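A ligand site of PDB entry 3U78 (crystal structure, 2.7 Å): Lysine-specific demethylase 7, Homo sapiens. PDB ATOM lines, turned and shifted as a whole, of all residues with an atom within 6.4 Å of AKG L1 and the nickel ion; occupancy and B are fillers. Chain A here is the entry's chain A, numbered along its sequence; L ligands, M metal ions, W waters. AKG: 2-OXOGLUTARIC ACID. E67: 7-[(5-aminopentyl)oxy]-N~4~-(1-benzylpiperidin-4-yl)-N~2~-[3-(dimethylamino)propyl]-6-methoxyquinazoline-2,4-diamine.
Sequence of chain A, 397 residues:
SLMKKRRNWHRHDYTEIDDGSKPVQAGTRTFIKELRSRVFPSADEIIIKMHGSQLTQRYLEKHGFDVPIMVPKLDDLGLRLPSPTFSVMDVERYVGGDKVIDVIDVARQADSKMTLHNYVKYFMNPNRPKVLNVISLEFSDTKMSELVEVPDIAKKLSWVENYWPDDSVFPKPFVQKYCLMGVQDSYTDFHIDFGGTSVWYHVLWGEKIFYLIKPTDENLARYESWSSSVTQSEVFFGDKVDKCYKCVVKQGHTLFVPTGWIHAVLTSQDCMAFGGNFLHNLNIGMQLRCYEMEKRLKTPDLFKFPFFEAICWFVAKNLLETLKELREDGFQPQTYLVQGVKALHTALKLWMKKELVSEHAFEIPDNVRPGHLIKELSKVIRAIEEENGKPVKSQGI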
ATOM      1  N   ASN A 133      -2.295  -8.901 -19.860  1.00  0.00           N
ATOM      2  CA  ASN A 133      -1.605  -9.507 -20.996  1.00  0.00           C
ATOM      3  C   ASN A 133      -2.509  -9.862 -22.166  1.00  0.00           C
ATOM      4  O   ASN A 133      -3.661 -10.255 -21.961  1.00  0.00           O
ATOM      5  CB  ASN A 133      -0.923 -10.776 -20.510  1.00  0.00           C
ATOM      6  CG  ASN A 133       0.341 -11.098 -21.286  1.00  0.00           C
ATOM      7  OD1 ASN A 133       0.781 -10.318 -22.141  1.00  0.00           O
ATOM      8  ND2 ASN A 133       0.936 -12.231 -20.981  1.00  0.00           N
ATOM      9  N   ILE A 135      -2.145 -12.448 -25.339  1.00  0.00           N
ATOM     10  CA  ILE A 135      -1.303 -13.469 -25.965  1.00  0.00           C
ATOM     11  C   ILE A 135      -2.016 -14.289 -27.033  1.00  0.00           C
ATOM     12  O   ILE A 135      -1.398 -15.152 -27.651  1.00  0.00           O
ATOM     13  CB  ILE A 135      -0.782 -14.451 -24.926  1.00  0.00           C
ATOM     14  CG1 ILE A 135      -1.873 -15.445 -24.560  1.00  0.00           C
ATOM     15  CG2 ILE A 135      -0.275 -13.722 -23.701  1.00  0.00           C
ATOM     16  CD1 ILE A 135      -1.611 -16.210 -23.267  1.00  0.00           C
ATOM     17  N   SER A 136      -3.304 -14.026 -27.256  1.00  0.00           N
ATOM     18  CA  SER A 136      -4.103 -14.875 -28.129  1.00  0.00           C
ATOM     19  C   SER A 136      -4.762 -14.144 -29.286  1.00  0.00           C
ATOM     20  O   SER A 136      -5.663 -14.691 -29.922  1.00  0.00           O
ATOM     21  CB  SER A 136      -5.192 -15.588 -27.321  1.00  0.00           C
ATOM     22  OG  SER A 136      -4.641 -16.612 -26.503  1.00  0.00           O
ATOM     23  N   LEU A 180       1.043 -10.383 -29.951  1.00  0.00           N
ATOM     24  CA  LEU A 180       1.117 -10.424 -28.501  1.00  0.00           C
ATOM     25  C   LEU A 180       1.555  -9.089 -27.967  1.00  0.00           C
ATOM     26  O   LEU A 180       2.644  -8.626 -28.275  1.00  0.00           O
ATOM     27  CB  LEU A 180       2.156 -11.433 -28.027  1.00  0.00           C
ATOM     28  CG  LEU A 180       1.926 -12.891 -28.366  1.00  0.00           C
ATOM     29  CD1 LEU A 180       2.394 -13.213 -29.792  1.00  0.00           C
ATOM     30  CD2 LEU A 180       2.631 -13.752 -27.337  1.00  0.00           C
ATOM     31  N   SER A 186       3.777  -9.122 -16.943  1.00  0.00           N
ATOM     32  CA  SER A 186       2.838 -10.112 -17.455  1.00  0.00           C
ATOM     33  C   SER A 186       3.520 -11.463 -17.333  1.00  0.00           C
ATOM     34  O   SER A 186       4.712 -11.600 -17.593  1.00  0.00           O
ATOM     35  CB  SER A 186       2.461  -9.865 -18.912  1.00  0.00           C
ATOM     36  OG  SER A 186       1.934  -8.565 -19.118  1.00  0.00           O
ATOM     37  N   TYR A 187       2.766 -12.473 -16.934  1.00  0.00           N
ATOM     38  CA  TYR A 187       3.339 -13.782 -16.753  1.00  0.00           C
ATOM     39  C   TYR A 187       2.340 -14.845 -17.176  1.00  0.00           C
ATOM     40  O   TYR A 187       1.190 -14.784 -16.791  1.00  0.00           O
ATOM     41  CB  TYR A 187       3.736 -13.985 -15.284  1.00  0.00           C
ATOM     42  CG  TYR A 187       4.092 -15.418 -14.940  1.00  0.00           C
ATOM     43  CD1 TYR A 187       5.259 -16.008 -15.424  1.00  0.00           C
ATOM     44  CD2 TYR A 187       3.261 -16.188 -14.158  1.00  0.00           C
ATOM     45  CE1 TYR A 187       5.596 -17.307 -15.116  1.00  0.00           C
ATOM     46  CE2 TYR A 187       3.582 -17.501 -13.841  1.00  0.00           C
ATOM     47  CZ  TYR A 187       4.741 -18.053 -14.321  1.00  0.00           C
ATOM     48  OH  TYR A 187       5.059 -19.347 -14.001  1.00  0.00           O
ATOM     49  N   THR A 188       2.779 -15.794 -17.993  1.00  0.00           N
ATOM     50  CA  THR A 188       1.933 -16.943 -18.283  1.00  0.00           C
ATOM     51  C   THR A 188       2.514 -18.189 -17.628  1.00  0.00           C
ATOM     52  O   THR A 188       3.707 -18.446 -17.729  1.00  0.00           O
ATOM     53  CB  THR A 188       1.766 -17.162 -19.773  1.00  0.00           C
ATOM     54  OG1 THR A 188       1.151 -16.005 -20.340  1.00  0.00           O
ATOM     55  CG2 THR A 188       0.886 -18.363 -20.022  1.00  0.00           C
ATOM     56  N   HIS A 191       2.458 -24.285 -19.351  1.00  0.00           N
ATOM     57  CA  HIS A 191       1.457 -25.023 -20.114  1.00  0.00           C
ATOM     58  C   HIS A 191       2.132 -25.700 -21.287  1.00  0.00           C
ATOM     59  O   HIS A 191       3.287 -25.442 -21.573  1.00  0.00           O
ATOM     60  CB  HIS A 191       0.436 -24.044 -20.654  1.00  0.00           C
ATOM     61  CG  HIS A 191       1.052 -22.966 -21.468  1.00  0.00           C
ATOM     62  ND1 HIS A 191       1.665 -21.875 -20.904  1.00  0.00           N
ATOM     63  CD2 HIS A 191       1.190 -22.832 -22.806  1.00  0.00           C
ATOM     64  CE1 HIS A 191       2.148 -21.097 -21.850  1.00  0.00           C
ATOM     65  NE2 HIS A 191       1.863 -21.654 -23.014  1.00  0.00           N
ATOM     66  N   ILE A 192       1.393 -26.569 -21.954  1.00  0.00           N
ATOM     67  CA  ILE A 192       1.864 -27.147 -23.198  1.00  0.00           C
ATOM     68  C   ILE A 192       0.943 -26.594 -24.258  1.00  0.00           C
ATOM     69  O   ILE A 192      -0.253 -26.533 -24.064  1.00  0.00           O
ATOM     70  CB  ILE A 192       1.765 -28.669 -23.176  1.00  0.00           C
ATOM     71  CG1 ILE A 192       2.747 -29.236 -22.161  1.00  0.00           C
ATOM     72  CG2 ILE A 192       2.074 -29.248 -24.526  1.00  0.00           C
ATOM     73  CD1 ILE A 192       2.601 -30.699 -21.919  1.00  0.00           C
ATOM     74  N   ASP A 193       1.492 -26.173 -25.387  1.00  0.00           N
ATOM     75  CA  ASP A 193       0.641 -25.505 -26.326  1.00  0.00           C
ATOM     76  C   ASP A 193      -0.474 -26.412 -26.800  1.00  0.00           C
ATOM     77  O   ASP A 193      -0.334 -27.641 -26.840  1.00  0.00           O
ATOM     78  CB  ASP A 193       1.443 -24.917 -27.468  1.00  0.00           C
ATOM     79  CG  ASP A 193       2.189 -23.691 -27.044  1.00  0.00           C
ATOM     80  OD1 ASP A 193       1.789 -23.126 -26.020  1.00  0.00           O
ATOM     81  OD2 ASP A 193       3.172 -23.284 -27.703  1.00  0.00           O
ATOM     82  N   PHE A 194      -1.612 -25.810 -27.117  1.00  0.00           N
ATOM     83  CA  PHE A 194      -2.761 -26.572 -27.561  1.00  0.00           C
ATOM     84  C   PHE A 194      -2.454 -27.579 -28.670  1.00  0.00           C
ATOM     85  O   PHE A 194      -1.801 -27.274 -29.663  1.00  0.00           O
ATOM     86  CB  PHE A 194      -3.877 -25.627 -27.970  1.00  0.00           C
ATOM     87  CG  PHE A 194      -3.552 -24.774 -29.150  1.00  0.00           C
ATOM     88  CD1 PHE A 194      -3.748 -25.249 -30.431  1.00  0.00           C
ATOM     89  CD2 PHE A 194      -3.063 -23.503 -28.962  1.00  0.00           C
ATOM     90  CE1 PHE A 194      -3.463 -24.455 -31.519  1.00  0.00           C
ATOM     91  CE2 PHE A 194      -2.773 -22.709 -30.042  1.00  0.00           C
ATOM     92  CZ  PHE A 194      -2.982 -23.186 -31.327  1.00  0.00           C
ATOM     93  N   VAL A 199       5.733 -23.812 -31.937  1.00  0.00           N
ATOM     94  CA  VAL A 199       5.517 -22.405 -32.164  1.00  0.00           C
ATOM     95  C   VAL A 199       6.757 -21.698 -32.633  1.00  0.00           C
ATOM     96  O   VAL A 199       7.877 -22.184 -32.466  1.00  0.00           O
ATOM     97  CB  VAL A 199       5.046 -21.666 -30.885  1.00  0.00           C
ATOM     98  CG1 VAL A 199       3.575 -21.882 -30.644  1.00  0.00           C
ATOM     99  CG2 VAL A 199       5.866 -22.091 -29.691  1.00  0.00           C
ATOM    100  N   TYR A 201       8.189 -17.597 -32.041  1.00  0.00           N
ATOM    101  CA  TYR A 201       7.904 -16.315 -31.444  1.00  0.00           C
ATOM    102  C   TYR A 201       8.979 -15.338 -31.871  1.00  0.00           C
ATOM    103  O   TYR A 201      10.151 -15.706 -31.937  1.00  0.00           O
ATOM    104  CB  TYR A 201       7.794 -16.411 -29.929  1.00  0.00           C
ATOM    105  CG  TYR A 201       6.457 -16.913 -29.452  1.00  0.00           C
ATOM    106  CD1 TYR A 201       6.306 -18.219 -28.970  1.00  0.00           C
ATOM    107  CD2 TYR A 201       5.327 -16.103 -29.501  1.00  0.00           C
ATOM    108  CE1 TYR A 201       5.065 -18.686 -28.535  1.00  0.00           C
ATOM    109  CE2 TYR A 201       4.083 -16.550 -29.064  1.00  0.00           C
ATOM    110  CZ  TYR A 201       3.949 -17.851 -28.590  1.00  0.00           C
ATOM    111  OH  TYR A 201       2.697 -18.289 -28.161  1.00  0.00           O
ATOM    112  N   LYS A 208      10.831 -10.887 -23.770  1.00  0.00           N
ATOM    113  CA  LYS A 208      10.097 -11.990 -23.143  1.00  0.00           C
ATOM    114  C   LYS A 208      11.120 -12.964 -22.638  1.00  0.00           C
ATOM    115  O   LYS A 208      12.196 -13.081 -23.210  1.00  0.00           O
ATOM    116  CB  LYS A 208       9.187 -12.693 -24.150  1.00  0.00           C
ATOM    117  CG  LYS A 208       8.033 -11.852 -24.617  1.00  0.00           C
ATOM    118  CD  LYS A 208       6.953 -12.709 -25.281  1.00  0.00           C
ATOM    119  CE  LYS A 208       5.604 -12.064 -25.085  1.00  0.00           C
ATOM    120  NZ  LYS A 208       5.462 -11.707 -23.643  1.00  0.00           N
ATOM    121  N   PHE A 210      11.412 -16.998 -21.640  1.00  0.00           N
ATOM    122  CA  PHE A 210      10.732 -18.288 -21.541  1.00  0.00           C
ATOM    123  C   PHE A 210      11.404 -19.185 -20.528  1.00  0.00           C
ATOM    124  O   PHE A 210      12.625 -19.222 -20.428  1.00  0.00           O
ATOM    125  CB  PHE A 210      10.720 -19.016 -22.887  1.00  0.00           C
ATOM    126  CG  PHE A 210       9.826 -18.389 -23.905  1.00  0.00           C
ATOM    127  CD1 PHE A 210       8.792 -19.125 -24.469  1.00  0.00           C
ATOM    128  CD2 PHE A 210      10.011 -17.086 -24.304  1.00  0.00           C
ATOM    129  CE1 PHE A 210       7.978 -18.573 -25.417  1.00  0.00           C
ATOM    130  CE2 PHE A 210       9.214 -16.521 -25.238  1.00  0.00           C
ATOM    131  CZ  PHE A 210       8.182 -17.267 -25.803  1.00  0.00           C
ATOM    132  N   HIS A 263       6.366 -24.790 -20.901  1.00  0.00           N
ATOM    133  CA  HIS A 263       6.984 -23.487 -20.761  1.00  0.00           C
ATOM    134  C   HIS A 263       6.095 -22.436 -20.121  1.00  0.00           C
ATOM    135  O   HIS A 263       4.890 -22.403 -20.344  1.00  0.00           O
ATOM    136  CB  HIS A 263       7.402 -22.986 -22.115  1.00  0.00           C
ATOM    137  CG  HIS A 263       6.258 -22.890 -23.076  1.00  0.00           C
ATOM    138  ND1 HIS A 263       5.692 -23.989 -23.665  1.00  0.00           N
ATOM    139  CD2 HIS A 263       5.581 -21.818 -23.541  1.00  0.00           C
ATOM    140  CE1 HIS A 263       4.712 -23.609 -24.466  1.00  0.00           C
ATOM    141  NE2 HIS A 263       4.637 -22.296 -24.416  1.00  0.00           N
ATOM    142  N   ALA A 264       6.724 -21.571 -19.338  1.00  0.00           N
ATOM    143  CA  ALA A 264       6.098 -20.389 -18.750  1.00  0.00           C
ATOM    144  C   ALA A 264       6.746 -19.213 -19.457  1.00  0.00           C
ATOM    145  O   ALA A 264       7.738 -19.397 -20.131  1.00  0.00           O
ATOM    146  CB  ALA A 264       6.364 -20.335 -17.245  1.00  0.00           C
ATOM    147  N   VAL A 265       6.197 -18.006 -19.320  1.00  0.00           N
ATOM    148  CA  VAL A 265       6.730 -16.845 -20.010  1.00  0.00           C
ATOM    149  C   VAL A 265       6.619 -15.620 -19.121  1.00  0.00           C
ATOM    150  O   VAL A 265       5.609 -15.438 -18.460  1.00  0.00           O
ATOM    151  CB  VAL A 265       5.982 -16.558 -21.311  1.00  0.00           C
ATOM    152  CG1 VAL A 265       6.478 -15.278 -21.946  1.00  0.00           C
ATOM    153  CG2 VAL A 265       6.099 -17.733 -22.271  1.00  0.00           C
ATOM    154  N   LEU A 266       7.656 -14.804 -19.094  1.00  0.00           N
ATOM    155  CA  LEU A 266       7.607 -13.562 -18.341  1.00  0.00           C
ATOM    156  C   LEU A 266       7.814 -12.400 -19.286  1.00  0.00           C
ATOM    157  O   LEU A 266       8.745 -12.397 -20.087  1.00  0.00           O
ATOM    158  CB  LEU A 266       8.652 -13.542 -17.224  1.00  0.00           C
ATOM    159  CG  LEU A 266       8.909 -12.214 -16.490  1.00  0.00           C
ATOM    160  CD1 LEU A 266       7.728 -11.844 -15.623  1.00  0.00           C
ATOM    161  CD2 LEU A 266      10.141 -12.310 -15.645  1.00  0.00           C
ATOM    162  N   THR A 267       6.948 -11.415 -19.216  1.00  0.00           N
ATOM    163  CA  THR A 267       7.093 -10.228 -20.026  1.00  0.00           C
ATOM    164  C   THR A 267       7.867  -9.239 -19.173  1.00  0.00           C
ATOM    165  O   THR A 267       7.287  -8.513 -18.359  1.00  0.00           O
ATOM    166  CB  THR A 267       5.706  -9.695 -20.469  1.00  0.00           C
ATOM    167  OG1 THR A 267       4.950 -10.776 -21.012  1.00  0.00           O
ATOM    168  CG2 THR A 267       5.842  -8.644 -21.557  1.00  0.00           C
ATOM    169  N   ASN A 277       1.340 -21.058 -34.485  1.00  0.00           N
ATOM    170  CA  ASN A 277       1.367 -22.454 -34.064  1.00  0.00           C
ATOM    171  C   ASN A 277       1.199 -23.384 -35.257  1.00  0.00           C
ATOM    172  O   ASN A 277       0.567 -23.026 -36.246  1.00  0.00           O
ATOM    173  CB  ASN A 277       0.258 -22.701 -33.041  1.00  0.00           C
ATOM    174  CG  ASN A 277       0.542 -22.028 -31.717  1.00  0.00           C
ATOM    175  OD1 ASN A 277       0.626 -20.799 -31.629  1.00  0.00           O
ATOM    176  ND2 ASN A 277       0.694 -22.841 -30.672  1.00  0.00           N
HETATM  177  C1  AKG L   1       1.369 -18.729 -25.335  1.00  0.00           C
HETATM  178  O1  AKG L   1       0.976 -19.883 -25.654  1.00  0.00           O
HETATM  179  O2  AKG L   1       0.541 -17.779 -25.342  1.00  0.00           O
HETATM  180  C2  AKG L   1       2.796 -18.470 -24.926  1.00  0.00           C
HETATM  181  O5  AKG L   1       3.467 -19.347 -24.378  1.00  0.00           O
HETATM  182  C3  AKG L   1       3.243 -17.041 -24.761  1.00  0.00           C
HETATM  183  C4  AKG L   1       2.821 -16.620 -23.396  1.00  0.00           C
HETATM  184  C5  AKG L   1       3.188 -15.189 -23.119  1.00  0.00           C
HETATM  185  O3  AKG L   1       4.002 -14.571 -23.858  1.00  0.00           O
HETATM  186  O4  AKG L   1       2.772 -14.630 -22.064  1.00  0.00           O
HETATM  187  N1  E67 L   2      -6.265 -22.533 -16.099  1.00  0.00           N
HETATM  188  C2  E67 L   2      -6.262 -23.269 -17.249  1.00  0.00           C
HETATM  189  N3  E67 L   2      -5.635 -22.826 -18.329  1.00  0.00           N
HETATM  190  C4  E67 L   2      -4.966 -21.665 -18.296  1.00  0.00           C
HETATM  191  C5  E67 L   2      -4.930 -20.894 -17.122  1.00  0.00           C
HETATM  192  C6  E67 L   2      -5.613 -21.374 -15.989  1.00  0.00           C
HETATM  193  CAA E67 L   2      -3.617 -20.015 -19.395  1.00  0.00           C
HETATM  194  CAB E67 L   2      -3.556 -19.236 -18.235  1.00  0.00           C
HETATM  195  CAC E67 L   2      -4.222 -19.663 -17.088  1.00  0.00           C
HETATM  196  CAF E67 L   2      -4.323 -21.236 -19.420  1.00  0.00           C
HETATM  197  OAK E67 L   2      -2.946 -19.678 -20.556  1.00  0.00           O
HETATM  198  OAL E67 L   2      -2.842 -18.033 -18.227  1.00  0.00           O
HETATM  199  CAM E67 L   2      -1.780 -17.879 -17.358  1.00  0.00           C
HETATM  200  NAN E67 L   2      -5.645 -20.644 -14.744  1.00  0.00           N
HETATM  201  NAU E67 L   2      -7.056 -24.491 -17.328  1.00  0.00           N
HETATM  202  CAV E67 L   2      -8.311 -25.254 -17.214  1.00  0.00           C
HETATM  203  CAW E67 L   2      -9.531 -24.419 -16.815  1.00  0.00           C
HETATM  204  CAX E67 L   2      -9.812 -23.127 -17.519  1.00  0.00           C
HETATM  205  NAY E67 L   2      -8.940 -21.982 -17.334  1.00  0.00           N
HETATM  206  CAZ E67 L   2      -9.631 -20.925 -16.563  1.00  0.00           C
HETATM  207  CBA E67 L   2      -8.539 -21.434 -18.588  1.00  0.00           C
HETATM  208  CBB E67 L   2      -2.079 -20.655 -21.071  1.00  0.00           C
HETATM  209  CBC E67 L   2      -2.311 -21.213 -22.502  1.00  0.00           C
HETATM  210  CBD E67 L   2      -2.206 -20.269 -23.699  1.00  0.00           C
HETATM  211  CBE E67 L   2      -2.144 -20.981 -25.051  1.00  0.00           C
HETATM  212  CBF E67 L   2      -1.820 -22.470 -25.008  1.00  0.00           C
HETATM  213  NBG E67 L   2      -1.795 -23.231 -26.260  1.00  0.00           N
HETATM  214 NI    NI M   1       2.655 -21.254 -25.083  1.00  0.00          NI
HETATM  215  O   HOH W   1       3.545 -20.797 -27.114  1.00  0.00           O
HETATM  216  O   HOH W   2       4.477 -13.247 -20.250  1.00  0.00           O
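The side-chain hydroxyl (OG1) of Thr 188 sits at hydrogen-bond distance from an oxygen (O4) of AKG L1 (2.7 Å).
NZ of Lys 208 is in salt-bridge range of O3 of AKG L1 (3.2 Å).
N of Phe 194 lies close to NBG of E67 L2 (2.7 Å).
O4 of AKG L1 sits at hydrogen-bond distance from ND2 of Asn 133 (3.2 Å).
OH of Tyr 201 lies close to O1 of AKG L1 (3.4 Å).
A nitrogen (NBG) of E67 L2 lies close to the side-chain carboxylate (OD1) of Asp 193, 3.6 Å away.
The side-chain hydroxyl (OG1) of Thr 267 is in hydrogen-bond range of the side-chain amino group (NZ) of Lys 208 (2.8 Å).
The backbone NH (N) of Thr 188 is in hydrogen-bond range of the backbone carbonyl oxygen (O) of Val 265 (2.9 Å).
Residues that only touch AKG L1: Val 265, Ile 135 and Leu 180.
Hydrophobic or aromatic side chains that line AKG L1: Ile 135, Leu 180, His 191, Tyr 201, His 263 and Val 265.
Of the 21 residues printed, 10 come within 4 Å of AKG L1.
The nickel ion is bound by an oxygen (O5) of AKG L1 (2.2 Å), an oxygen (O1) of AKG L1 (2.2 Å), a ring nitrogen (NE2) of His 191 (2.3 Å), water W1 (2.3 Å), the side-chain carboxylate (OD1) of Asp 193 (2.3 Å) and a ring nitrogen (NE2) of His 263 (2.3 Å).
The nickel ion has six donor atoms within binding distance.
Water W1 bridges OD2 of Asp 193 (2.6 Å) and OH of Tyr 201 (2.8 Å).
Water W2 lies within hydrogen-bond range of the side-chain hydroxyl (OG1) of Thr 267 (2.6 Å), an oxygen (O4) of AKG L1 (2.8 Å), the backbone carbonyl oxygen (O) of Val 265 (3.0 Å) and the backbone carbonyl oxygen (O) of Ser 186 (3.1 Å).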
